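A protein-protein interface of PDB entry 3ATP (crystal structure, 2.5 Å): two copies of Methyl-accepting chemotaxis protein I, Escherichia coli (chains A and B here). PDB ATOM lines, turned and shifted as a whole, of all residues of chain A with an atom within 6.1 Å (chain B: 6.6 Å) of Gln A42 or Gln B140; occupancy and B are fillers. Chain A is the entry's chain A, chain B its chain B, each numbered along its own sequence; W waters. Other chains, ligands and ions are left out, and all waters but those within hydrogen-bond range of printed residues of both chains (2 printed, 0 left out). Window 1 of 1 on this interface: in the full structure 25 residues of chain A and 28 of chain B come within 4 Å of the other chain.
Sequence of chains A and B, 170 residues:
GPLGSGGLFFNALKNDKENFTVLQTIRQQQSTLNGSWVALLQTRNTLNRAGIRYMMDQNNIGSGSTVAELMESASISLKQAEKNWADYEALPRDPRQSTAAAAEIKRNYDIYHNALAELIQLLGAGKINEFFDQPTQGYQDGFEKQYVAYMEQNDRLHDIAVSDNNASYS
Gln B140 touches one residue of chain A. Printed residues of chain A within 4 Å of Arg B44: Asn A45 (2.9 Å). Printed residues of chain A within 4 Å of Asn B45: Arg A44 and Asn A45. Of the printed residues of chain A, Glu B144 touches Gln A42 (3.2 Å). Of the printed residues of chain B, Val A38 touches Trp B37 (3.5 Å). Printed residues of chain B within 4 Å of Asn A45: Arg B44 (2.9 Å) and Asn B45 (3.1 Å).
Water W2 bridges OD1 of Asn B45 (2.9 Å) and NH1 of Arg A44 (3.4 Å). Water W1 lies within hydrogen-bond range of the side-chain amide nitrogen (NE2) of Gln B140, the side-chain amide oxygen (OD1) of Asn A45 and the guanidinium group (NH1) of Arg B44.
OE1 of Glu B144 sits at hydrogen-bond distance from NE2 of Gln A42 (3.2 Å). The backbone NH (N) of Asn A45 lies close to the side-chain amide nitrogen (ND2) of Asn B45. The side-chain amide oxygen (OD1) of Asn A45 sits at hydrogen-bond distance from the guanidinium group (NE) of Arg B44. The backbone carbonyl oxygen (O) of Arg A44 lies close to the side-chain amide nitrogen (ND2) of Asn B45, at 3.3 Å.
Hydrophobic or aromatic side chains of chain B within 4 Å of the printed part of chain A: Trp B37. Printed residues of chain A that touch a printed residue of chain B: Val A38, Gln A42, Arg A44 and Asn A45. Hydrophobic or aromatic side chains of chain A that line the printed part of chain B: Val A38. Along chain A the printed residues that touch a printed residue of chain B span positions 38 to 45. Among the printed residues, 7 pairs touch across the chains. Among the printed residues, no Asp or Glu carboxylate lies within 4 Å of a Lys or Arg side-chain nitrogen of the other chain.
Arg A44 touches Asn B45, and with the chains exchanged Asn A45 touches Arg B44. Asn B45 touches its own counterpart, Asn A45. Positions printed for both chains: 37, 40, 41, 44 and 45.
Among the printed residues, pairs that only touch across the chains: Gln A42 with Trp B37 (3.5 Å), Val A38 with Trp B37 (3.5 Å) and Gln A42 with Gln B140 (3.8 Å).
NH1 of Arg B44 is in hydrogen-bond range of OE1 of Gln B137, 3.1 Å away. NH1 of Arg B44 is in hydrogen-bond range of OE1 of Gln B140 (2.9 Å). O of Gln A42 is in hydrogen-bond range of OG1 of Thr A46, at 3.2 Å. The side-chain hydroxyl of Tyr B112 is in hydrogen-bond range of the side-chain amide oxygen of Gln B140 (2.6 Å).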
ATOM      1  N   TRP A  37      15.375 -15.681  24.443  1.00  0.00           N
ATOM      2  CA  TRP A  37      15.136 -15.884  23.011  1.00  0.00           C
ATOM      3  C   TRP A  37      16.459 -16.171  22.331  1.00  0.00           C
ATOM      4  O   TRP A  37      16.638 -17.214  21.703  1.00  0.00           O
ATOM      5  CB  TRP A  37      14.527 -14.615  22.407  1.00  0.00           C
ATOM      6  CG  TRP A  37      14.154 -14.654  20.933  1.00  0.00           C
ATOM      7  CD1 TRP A  37      14.039 -13.574  20.100  1.00  0.00           C
ATOM      8  CD2 TRP A  37      13.769 -15.804  20.149  1.00  0.00           C
ATOM      9  NE1 TRP A  37      13.603 -13.976  18.853  1.00  0.00           N
ATOM     10  CE2 TRP A  37      13.436 -15.333  18.854  1.00  0.00           C
ATOM     11  CE3 TRP A  37      13.675 -17.175  20.412  1.00  0.00           C
ATOM     12  CZ2 TRP A  37      13.016 -16.188  17.837  1.00  0.00           C
ATOM     13  CZ3 TRP A  37      13.251 -18.020  19.398  1.00  0.00           C
ATOM     14  CH2 TRP A  37      12.932 -17.522  18.127  1.00  0.00           C
ATOM     15  N   VAL A  38      17.390 -15.236  22.469  1.00  0.00           N
ATOM     16  CA  VAL A  38      18.700 -15.373  21.850  1.00  0.00           C
ATOM     17  C   VAL A  38      19.356 -16.683  22.331  1.00  0.00           C
ATOM     18  O   VAL A  38      19.907 -17.444  21.518  1.00  0.00           O
ATOM     19  CB  VAL A  38      19.615 -14.182  22.203  1.00  0.00           C
ATOM     20  CG1 VAL A  38      21.051 -14.595  22.071  1.00  0.00           C
ATOM     21  CG2 VAL A  38      19.296 -13.012  21.271  1.00  0.00           C
ATOM     22  N   ALA A  39      19.334 -16.951  23.638  1.00  0.00           N
ATOM     23  CA  ALA A  39      19.975 -18.168  24.132  1.00  0.00           C
ATOM     24  C   ALA A  39      19.419 -19.485  23.590  1.00  0.00           C
ATOM     25  O   ALA A  39      20.178 -20.458  23.417  1.00  0.00           O
ATOM     26  CB  ALA A  39      19.975 -18.180  25.652  1.00  0.00           C
ATOM     27  N   LEU A  40      18.117 -19.519  23.323  1.00  0.00           N
ATOM     28  CA  LEU A  40      17.545 -20.731  22.779  1.00  0.00           C
ATOM     29  C   LEU A  40      18.069 -20.889  21.360  1.00  0.00           C
ATOM     30  O   LEU A  40      18.375 -21.994  20.896  1.00  0.00           O
ATOM     31  CB  LEU A  40      16.041 -20.607  22.732  1.00  0.00           C
ATOM     32  CG  LEU A  40      15.242 -20.380  24.006  1.00  0.00           C
ATOM     33  CD1 LEU A  40      14.125 -19.424  23.685  1.00  0.00           C
ATOM     34  CD2 LEU A  40      14.711 -21.679  24.549  1.00  0.00           C
ATOM     35  N   LEU A  41      18.136 -19.754  20.678  1.00  0.00           N
ATOM     36  CA  LEU A  41      18.609 -19.697  19.305  1.00  0.00           C
ATOM     37  C   LEU A  41      20.079 -20.071  19.201  1.00  0.00           C
ATOM     38  O   LEU A  41      20.503 -20.716  18.242  1.00  0.00           O
ATOM     39  CB  LEU A  41      18.418 -18.291  18.749  1.00  0.00           C
ATOM     40  CG  LEU A  41      17.041 -17.925  18.225  1.00  0.00           C
ATOM     41  CD1 LEU A  41      16.984 -16.428  18.036  1.00  0.00           C
ATOM     42  CD2 LEU A  41      16.766 -18.647  16.924  1.00  0.00           C
ATOM     43  N   GLN A  42      20.880 -19.645  20.164  1.00  0.00           N
ATOM     44  CA  GLN A  42      22.287 -20.001  20.096  1.00  0.00           C
ATOM     45  C   GLN A  42      22.406 -21.478  20.404  1.00  0.00           C
ATOM     46  O   GLN A  42      23.267 -22.170  19.861  1.00  0.00           O
ATOM     47  CB  GLN A  42      23.108 -19.179  21.082  1.00  0.00           C
ATOM     48  CG  GLN A  42      23.778 -17.993  20.415  1.00  0.00           C
ATOM     49  CD  GLN A  42      24.032 -16.875  21.388  1.00  0.00           C
ATOM     50  OE1 GLN A  42      23.730 -17.012  22.578  1.00  0.00           O
ATOM     51  NE2 GLN A  42      24.582 -15.757  20.902  1.00  0.00           N
ATOM     52  N   THR A  43      21.513 -21.959  21.260  1.00  0.00           N
ATOM     53  CA  THR A  43      21.524 -23.355  21.626  1.00  0.00           C
ATOM     54  C   THR A  43      21.214 -24.229  20.421  1.00  0.00           C
ATOM     55  O   THR A  43      21.903 -25.210  20.151  1.00  0.00           O
ATOM     56  CB  THR A  43      20.478 -23.669  22.694  1.00  0.00           C
ATOM     57  OG1 THR A  43      20.749 -22.914  23.877  1.00  0.00           O
ATOM     58  CG2 THR A  43      20.523 -25.149  23.038  1.00  0.00           C
ATOM     59  N   ARG A  44      20.166 -23.863  19.702  1.00  0.00           N
ATOM     60  CA  ARG A  44      19.747 -24.619  18.541  1.00  0.00           C
ATOM     61  C   ARG A  44      20.881 -24.757  17.538  1.00  0.00           C
ATOM     62  O   ARG A  44      21.155 -25.853  17.044  1.00  0.00           O
ATOM     63  CB  ARG A  44      18.565 -23.941  17.862  1.00  0.00           C
ATOM     64  CG  ARG A  44      17.728 -24.917  17.076  1.00  0.00           C
ATOM     65  CD  ARG A  44      16.841 -24.223  16.111  1.00  0.00           C
ATOM     66  NE  ARG A  44      16.327 -25.161  15.127  1.00  0.00           N
ATOM     67  CZ  ARG A  44      15.464 -24.827  14.174  1.00  0.00           C
ATOM     68  NH1 ARG A  44      15.031 -23.577  14.090  1.00  0.00           N
ATOM     69  NH2 ARG A  44      15.016 -25.732  13.318  1.00  0.00           N
ATOM     70  N   ASN A  45      21.526 -23.638  17.232  1.00  0.00           N
ATOM     71  CA  ASN A  45      22.630 -23.629  16.279  1.00  0.00           C
ATOM     72  C   ASN A  45      23.826 -24.435  16.743  1.00  0.00           C
ATOM     73  O   ASN A  45      24.510 -25.063  15.923  1.00  0.00           O
ATOM     74  CB  ASN A  45      23.090 -22.204  15.993  1.00  0.00           C
ATOM     75  CG  ASN A  45      24.274 -22.170  15.049  1.00  0.00           C
ATOM     76  OD1 ASN A  45      25.379 -21.773  15.425  1.00  0.00           O
ATOM     77  ND2 ASN A  45      24.060 -22.631  13.821  1.00  0.00           N
ATOM     78  N   THR A  46      24.102 -24.397  18.040  1.00  0.00           N
ATOM     79  CA  THR A  46      25.216 -25.156  18.568  1.00  0.00           C
ATOM     80  C   THR A  46      24.883 -26.622  18.372  1.00  0.00           C
ATOM     81  O   THR A  46      25.622 -27.359  17.712  1.00  0.00           O
ATOM     82  CB  THR A  46      25.406 -24.890  20.044  1.00  0.00           C
ATOM     83  OG1 THR A  46      26.113 -23.656  20.211  1.00  0.00           O
ATOM     84  CG2 THR A  46      26.170 -26.032  20.694  1.00  0.00           C
ATOM     85  N   LEU A  47      23.756 -27.028  18.952  1.00  0.00           N
ATOM     86  CA  LEU A  47      23.287 -28.395  18.852  1.00  0.00           C
ATOM     87  C   LEU A  47      23.432 -28.844  17.408  1.00  0.00           C
ATOM     88  O   LEU A  47      23.671 -30.020  17.139  1.00  0.00           O
ATOM     89  CB  LEU A  47      21.817 -28.485  19.259  1.00  0.00           C
ATOM     90  CG  LEU A  47      21.441 -28.253  20.719  1.00  0.00           C
ATOM     91  CD1 LEU A  47      19.969 -28.497  20.916  1.00  0.00           C
ATOM     92  CD2 LEU A  47      22.225 -29.204  21.586  1.00  0.00           C
ATOM     93  N   SER A  77      24.409 -22.845  27.486  1.00  0.00           N
ATOM     94  CA  SER A  77      23.549 -21.827  26.884  1.00  0.00           C
ATOM     95  C   SER A  77      22.049 -22.042  27.091  1.00  0.00           C
ATOM     96  O   SER A  77      21.291 -21.074  27.233  1.00  0.00           O
ATOM     97  CB  SER A  77      23.858 -21.708  25.393  1.00  0.00           C
ATOM     98  OG  SER A  77      23.793 -22.978  24.778  1.00  0.00           O
ATOM     99  N   TRP B  37      20.252  -9.041  14.408  1.00  0.00           N
ATOM    100  CA  TRP B  37      21.070  -9.950  15.180  1.00  0.00           C
ATOM    101  C   TRP B  37      20.329 -11.299  15.182  1.00  0.00           C
ATOM    102  O   TRP B  37      20.909 -12.334  14.913  1.00  0.00           O
ATOM    103  CB  TRP B  37      21.243  -9.383  16.600  1.00  0.00           C
ATOM    104  CG  TRP B  37      21.751 -10.335  17.661  1.00  0.00           C
ATOM    105  CD1 TRP B  37      21.247 -10.481  18.916  1.00  0.00           C
ATOM    106  CD2 TRP B  37      22.879 -11.225  17.577  1.00  0.00           C
ATOM    107  NE1 TRP B  37      21.987 -11.397  19.626  1.00  0.00           N
ATOM    108  CE2 TRP B  37      22.988 -11.868  18.831  1.00  0.00           C
ATOM    109  CE3 TRP B  37      23.799 -11.534  16.571  1.00  0.00           C
ATOM    110  CZ2 TRP B  37      23.987 -12.809  19.096  1.00  0.00           C
ATOM    111  CZ3 TRP B  37      24.794 -12.471  16.841  1.00  0.00           C
ATOM    112  CH2 TRP B  37      24.876 -13.096  18.094  1.00  0.00           C
ATOM    113  N   LEU B  40      20.577 -13.174  11.952  1.00  0.00           N
ATOM    114  CA  LEU B  40      21.899 -13.681  11.641  1.00  0.00           C
ATOM    115  C   LEU B  40      22.039 -15.074  12.249  1.00  0.00           C
ATOM    116  O   LEU B  40      22.618 -15.966  11.635  1.00  0.00           O
ATOM    117  CB  LEU B  40      22.987 -12.729  12.171  1.00  0.00           C
ATOM    118  CG  LEU B  40      23.087 -11.401  11.399  1.00  0.00           C
ATOM    119  CD1 LEU B  40      23.946 -10.404  12.142  1.00  0.00           C
ATOM    120  CD2 LEU B  40      23.669 -11.650  10.015  1.00  0.00           C
ATOM    121  N   LEU B  41      21.490 -15.258  13.447  1.00  0.00           N
ATOM    122  CA  LEU B  41      21.553 -16.543  14.127  1.00  0.00           C
ATOM    123  C   LEU B  41      20.674 -17.576  13.445  1.00  0.00           C
ATOM    124  O   LEU B  41      21.055 -18.733  13.281  1.00  0.00           O
ATOM    125  CB  LEU B  41      21.101 -16.389  15.577  1.00  0.00           C
ATOM    126  CG  LEU B  41      21.976 -15.485  16.438  1.00  0.00           C
ATOM    127  CD1 LEU B  41      21.190 -15.060  17.667  1.00  0.00           C
ATOM    128  CD2 LEU B  41      23.262 -16.207  16.816  1.00  0.00           C
ATOM    129  N   ARG B  44      22.492 -18.628  10.481  1.00  0.00           N
ATOM    130  CA  ARG B  44      23.605 -19.481  10.789  1.00  0.00           C
ATOM    131  C   ARG B  44      23.042 -20.885  11.074  1.00  0.00           C
ATOM    132  O   ARG B  44      23.508 -21.883  10.516  1.00  0.00           O
ATOM    133  CB  ARG B  44      24.339 -18.951  12.002  1.00  0.00           C
ATOM    134  CG  ARG B  44      25.712 -19.549  12.124  1.00  0.00           C
ATOM    135  CD  ARG B  44      26.260 -19.423  13.524  1.00  0.00           C
ATOM    136  NE  ARG B  44      27.297 -20.420  13.769  1.00  0.00           N
ATOM    137  CZ  ARG B  44      28.065 -20.454  14.855  1.00  0.00           C
ATOM    138  NH1 ARG B  44      27.918 -19.544  15.808  1.00  0.00           N
ATOM    139  NH2 ARG B  44      28.994 -21.399  14.987  1.00  0.00           N
ATOM    140  N   ASN B  45      22.021 -20.956  11.926  1.00  0.00           N
ATOM    141  CA  ASN B  45      21.414 -22.236  12.273  1.00  0.00           C
ATOM    142  C   ASN B  45      20.938 -23.025  11.062  1.00  0.00           C
ATOM    143  O   ASN B  45      21.295 -24.196  10.865  1.00  0.00           O
ATOM    144  CB  ASN B  45      20.231 -22.029  13.223  1.00  0.00           C
ATOM    145  CG  ASN B  45      19.496 -23.334  13.530  1.00  0.00           C
ATOM    146  OD1 ASN B  45      18.544 -23.746  12.838  1.00  0.00           O
ATOM    147  ND2 ASN B  45      19.959 -24.008  14.555  1.00  0.00           N
ATOM    148  N   ASN B 108      31.981  -5.459  12.702  1.00  0.00           N
ATOM    149  CA  ASN B 108      31.755  -6.834  13.157  1.00  0.00           C
ATOM    150  C   ASN B 108      30.504  -7.417  12.487  1.00  0.00           C
ATOM    151  O   ASN B 108      30.397  -8.633  12.284  1.00  0.00           O
ATOM    152  CB  ASN B 108      31.611  -6.869  14.677  1.00  0.00           C
ATOM    153  CG  ASN B 108      32.894  -6.465  15.402  1.00  0.00           C
ATOM    154  OD1 ASN B 108      33.881  -6.093  14.786  1.00  0.00           O
ATOM    155  ND2 ASN B 108      32.870  -6.533  16.726  1.00  0.00           N
ATOM    156  N   ILE B 111      31.585  -8.409   8.771  1.00  0.00           N
ATOM    157  CA  ILE B 111      32.374  -9.637   8.688  1.00  0.00           C
ATOM    158  C   ILE B 111      31.562 -10.873   9.064  1.00  0.00           C
ATOM    159  O   ILE B 111      31.683 -11.924   8.434  1.00  0.00           O
ATOM    160  CB  ILE B 111      33.696  -9.522   9.546  1.00  0.00           C
ATOM    161  CG1 ILE B 111      33.855 -10.701  10.504  1.00  0.00           C
ATOM    162  CG2 ILE B 111      33.705  -8.231  10.338  1.00  0.00           C
ATOM    163  CD1 ILE B 111      34.909 -10.430  11.593  1.00  0.00           C
ATOM    164  N   TYR B 112      30.717 -10.744  10.080  1.00  0.00           N
ATOM    165  CA  TYR B 112      29.889 -11.868  10.496  1.00  0.00           C
ATOM    166  C   TYR B 112      28.899 -12.128   9.372  1.00  0.00           C
ATOM    167  O   TYR B 112      28.700 -13.275   8.959  1.00  0.00           O
ATOM    168  CB  TYR B 112      29.145 -11.538  11.795  1.00  0.00           C
ATOM    169  CG  TYR B 112      28.202 -12.629  12.268  1.00  0.00           C
ATOM    170  CD1 TYR B 112      28.468 -13.981  11.995  1.00  0.00           C
ATOM    171  CD2 TYR B 112      27.051 -12.318  13.009  1.00  0.00           C
ATOM    172  CE1 TYR B 112      27.611 -14.996  12.445  1.00  0.00           C
ATOM    173  CE2 TYR B 112      26.189 -13.327  13.464  1.00  0.00           C
ATOM    174  CZ  TYR B 112      26.475 -14.659  13.178  1.00  0.00           C
ATOM    175  OH  TYR B 112      25.632 -15.652  13.624  1.00  0.00           O
ATOM    176  N   LEU B 116      28.796 -15.596   6.745  1.00  0.00           N
ATOM    177  CA  LEU B 116      27.646 -16.435   6.387  1.00  0.00           C
ATOM    178  C   LEU B 116      27.277 -16.444   4.900  1.00  0.00           C
ATOM    179  O   LEU B 116      26.871 -17.472   4.365  1.00  0.00           O
ATOM    180  CB  LEU B 116      26.407 -16.021   7.167  1.00  0.00           C
ATOM    181  CG  LEU B 116      26.411 -15.991   8.695  1.00  0.00           C
ATOM    182  CD1 LEU B 116      24.991 -16.186   9.159  1.00  0.00           C
ATOM    183  CD2 LEU B 116      27.338 -17.014   9.294  1.00  0.00           C
ATOM    184  N   PRO B 135      35.945 -19.890  10.872  1.00  0.00           N
ATOM    185  CA  PRO B 135      35.892 -19.365  12.238  1.00  0.00           C
ATOM    186  C   PRO B 135      34.605 -18.579  12.446  1.00  0.00           C
ATOM    187  O   PRO B 135      34.632 -17.413  12.844  1.00  0.00           O
ATOM    188  CB  PRO B 135      37.127 -18.479  12.305  1.00  0.00           C
ATOM    189  CG  PRO B 135      37.221 -17.964  10.911  1.00  0.00           C
ATOM    190  CD  PRO B 135      36.993 -19.210  10.097  1.00  0.00           C
ATOM    191  N   THR B 136      33.477 -19.219  12.172  1.00  0.00           N
ATOM    192  CA  THR B 136      32.199 -18.550  12.323  1.00  0.00           C
ATOM    193  C   THR B 136      31.928 -18.276  13.783  1.00  0.00           C
ATOM    194  O   THR B 136      31.647 -17.138  14.149  1.00  0.00           O
ATOM    195  CB  THR B 136      31.080 -19.416  11.867  1.00  0.00           C
ATOM    196  OG1 THR B 136      31.239 -19.736  10.478  1.00  0.00           O
ATOM    197  CG2 THR B 136      29.695 -18.742  12.147  1.00  0.00           C
ATOM    198  N   GLN B 137      32.010 -19.311  14.619  1.00  0.00           N
ATOM    199  CA  GLN B 137      31.766 -19.106  16.028  1.00  0.00           C
ATOM    200  C   GLN B 137      32.585 -17.917  16.518  1.00  0.00           C
ATOM    201  O   GLN B 137      32.206 -17.263  17.487  1.00  0.00           O
ATOM    202  CB  GLN B 137      32.106 -20.368  16.822  1.00  0.00           C
ATOM    203  CG  GLN B 137      31.827 -20.244  18.325  1.00  0.00           C
ATOM    204  CD  GLN B 137      30.518 -19.524  18.639  1.00  0.00           C
ATOM    205  OE1 GLN B 137      29.426 -20.074  18.482  1.00  0.00           O
ATOM    206  NE2 GLN B 137      30.632 -18.280  19.078  1.00  0.00           N
ATOM    207  N   GLY B 138      33.687 -17.621  15.828  1.00  0.00           N
ATOM    208  CA  GLY B 138      34.526 -16.500  16.214  1.00  0.00           C
ATOM    209  C   GLY B 138      33.963 -15.163  15.761  1.00  0.00           C
ATOM    210  O   GLY B 138      33.882 -14.211  16.540  1.00  0.00           O
ATOM    211  N   TYR B 139      33.568 -15.095  14.493  1.00  0.00           N
ATOM    212  CA  TYR B 139      33.014 -13.871  13.909  1.00  0.00           C
ATOM    213  C   TYR B 139      31.733 -13.408  14.597  1.00  0.00           C
ATOM    214  O   TYR B 139      31.423 -12.206  14.612  1.00  0.00           O
ATOM    215  CB  TYR B 139      32.702 -14.084  12.431  1.00  0.00           C
ATOM    216  CG  TYR B 139      33.904 -14.404  11.575  1.00  0.00           C
ATOM    217  CD1 TYR B 139      35.029 -13.590  11.597  1.00  0.00           C
ATOM    218  CD2 TYR B 139      33.902 -15.509  10.725  1.00  0.00           C
ATOM    219  CE1 TYR B 139      36.129 -13.861  10.797  1.00  0.00           C
ATOM    220  CE2 TYR B 139      34.993 -15.795   9.920  1.00  0.00           C
ATOM    221  CZ  TYR B 139      36.109 -14.961   9.959  1.00  0.00           C
ATOM    222  OH  TYR B 139      37.205 -15.218   9.167  1.00  0.00           O
ATOM    223  N   GLN B 140      30.995 -14.369  15.155  1.00  0.00           N
ATOM    224  CA  GLN B 140      29.733 -14.097  15.823  1.00  0.00           C
ATOM    225  C   GLN B 140      29.875 -13.348  17.138  1.00  0.00           C
ATOM    226  O   GLN B 140      29.329 -12.259  17.284  1.00  0.00           O
ATOM    227  CB  GLN B 140      28.970 -15.396  16.042  1.00  0.00           C
ATOM    228  CG  GLN B 140      27.590 -15.200  16.657  1.00  0.00           C
ATOM    229  CD  GLN B 140      26.800 -16.485  16.705  1.00  0.00           C
ATOM    230  OE1 GLN B 140      26.451 -17.043  15.670  1.00  0.00           O
ATOM    231  NE2 GLN B 140      26.521 -16.966  17.909  1.00  0.00           N
ATOM    232  N   ASP B 141      30.576 -13.914  18.112  1.00  0.00           N
ATOM    233  CA  ASP B 141      30.745 -13.180  19.365  1.00  0.00           C
ATOM    234  C   ASP B 141      31.538 -11.944  19.014  1.00  0.00           C
ATOM    235  O   ASP B 141      31.591 -10.992  19.781  1.00  0.00           O
ATOM    236  CB  ASP B 141      31.489 -14.008  20.390  1.00  0.00           C
ATOM    237  CG  ASP B 141      31.840 -15.356  19.864  1.00  0.00           C
ATOM    238  OD1 ASP B 141      32.506 -15.388  18.808  1.00  0.00           O
ATOM    239  OD2 ASP B 141      31.450 -16.363  20.494  1.00  0.00           O
ATOM    240  N   GLY B 142      32.166 -11.969  17.844  1.00  0.00           N
ATOM    241  CA  GLY B 142      32.891 -10.797  17.415  1.00  0.00           C
ATOM    242  C   GLY B 142      31.785  -9.767  17.354  1.00  0.00           C
ATOM    243  O   GLY B 142      31.870  -8.699  17.966  1.00  0.00           O
ATOM    244  N   PHE B 143      30.719 -10.122  16.640  1.00  0.00           N
ATOM    245  CA  PHE B 143      29.561  -9.254  16.507  1.00  0.00           C
ATOM    246  C   PHE B 143      28.808  -9.105  17.828  1.00  0.00           C
ATOM    247  O   PHE B 143      28.595  -7.989  18.309  1.00  0.00           O
ATOM    248  CB  PHE B 143      28.584  -9.797  15.452  1.00  0.00           C
ATOM    249  CG  PHE B 143      27.318  -8.989  15.334  1.00  0.00           C
ATOM    250  CD1 PHE B 143      26.161  -9.357  16.009  1.00  0.00           C
ATOM    251  CD2 PHE B 143      27.293  -7.845  14.560  1.00  0.00           C
ATOM    252  CE1 PHE B 143      25.005  -8.596  15.908  1.00  0.00           C
ATOM    253  CE2 PHE B 143      26.141  -7.086  14.460  1.00  0.00           C
ATOM    254  CZ  PHE B 143      24.998  -7.467  15.135  1.00  0.00           C
ATOM    255  N   GLU B 144      28.390 -10.233  18.397  1.00  0.00           N
ATOM    256  CA  GLU B 144      27.638 -10.223  19.648  1.00  0.00           C
ATOM    257  C   GLU B 144      28.325  -9.391  20.721  1.00  0.00           C
ATOM    258  O   GLU B 144      27.721  -8.997  21.708  1.00  0.00           O
ATOM    259  CB  GLU B 144      27.435 -11.653  20.165  1.00  0.00           C
ATOM    260  CG  GLU B 144      26.964 -11.726  21.614  1.00  0.00           C
ATOM    261  CD  GLU B 144      26.644 -13.133  22.076  1.00  0.00           C
ATOM    262  OE1 GLU B 144      27.212 -14.103  21.527  1.00  0.00           O
ATOM    263  OE2 GLU B 144      25.825 -13.269  23.010  1.00  0.00           O
ATOM    264  N   LYS B 145      29.595  -9.104  20.524  1.00  0.00           N
ATOM    265  CA  LYS B 145      30.325  -8.339  21.514  1.00  0.00           C
ATOM    266  C   LYS B 145      30.083  -6.824  21.444  1.00  0.00           C
ATOM    267  O   LYS B 145      30.074  -6.154  22.467  1.00  0.00           O
ATOM    268  CB  LYS B 145      31.799  -8.668  21.366  1.00  0.00           C
ATOM    269  CG  LYS B 145      32.656  -8.134  22.436  1.00  0.00           C
ATOM    270  CD  LYS B 145      33.928  -7.622  21.809  1.00  0.00           C
ATOM    271  CE  LYS B 145      34.720  -6.860  22.830  1.00  0.00           C
ATOM    272  NZ  LYS B 145      33.805  -5.998  23.653  1.00  0.00           N
HETATM  273  O   HOH W   1      25.617 -20.102  18.260  1.00  0.00           O
HETATM  274  O   HOH W   2      16.937 -21.405  12.336  1.00  0.00           O
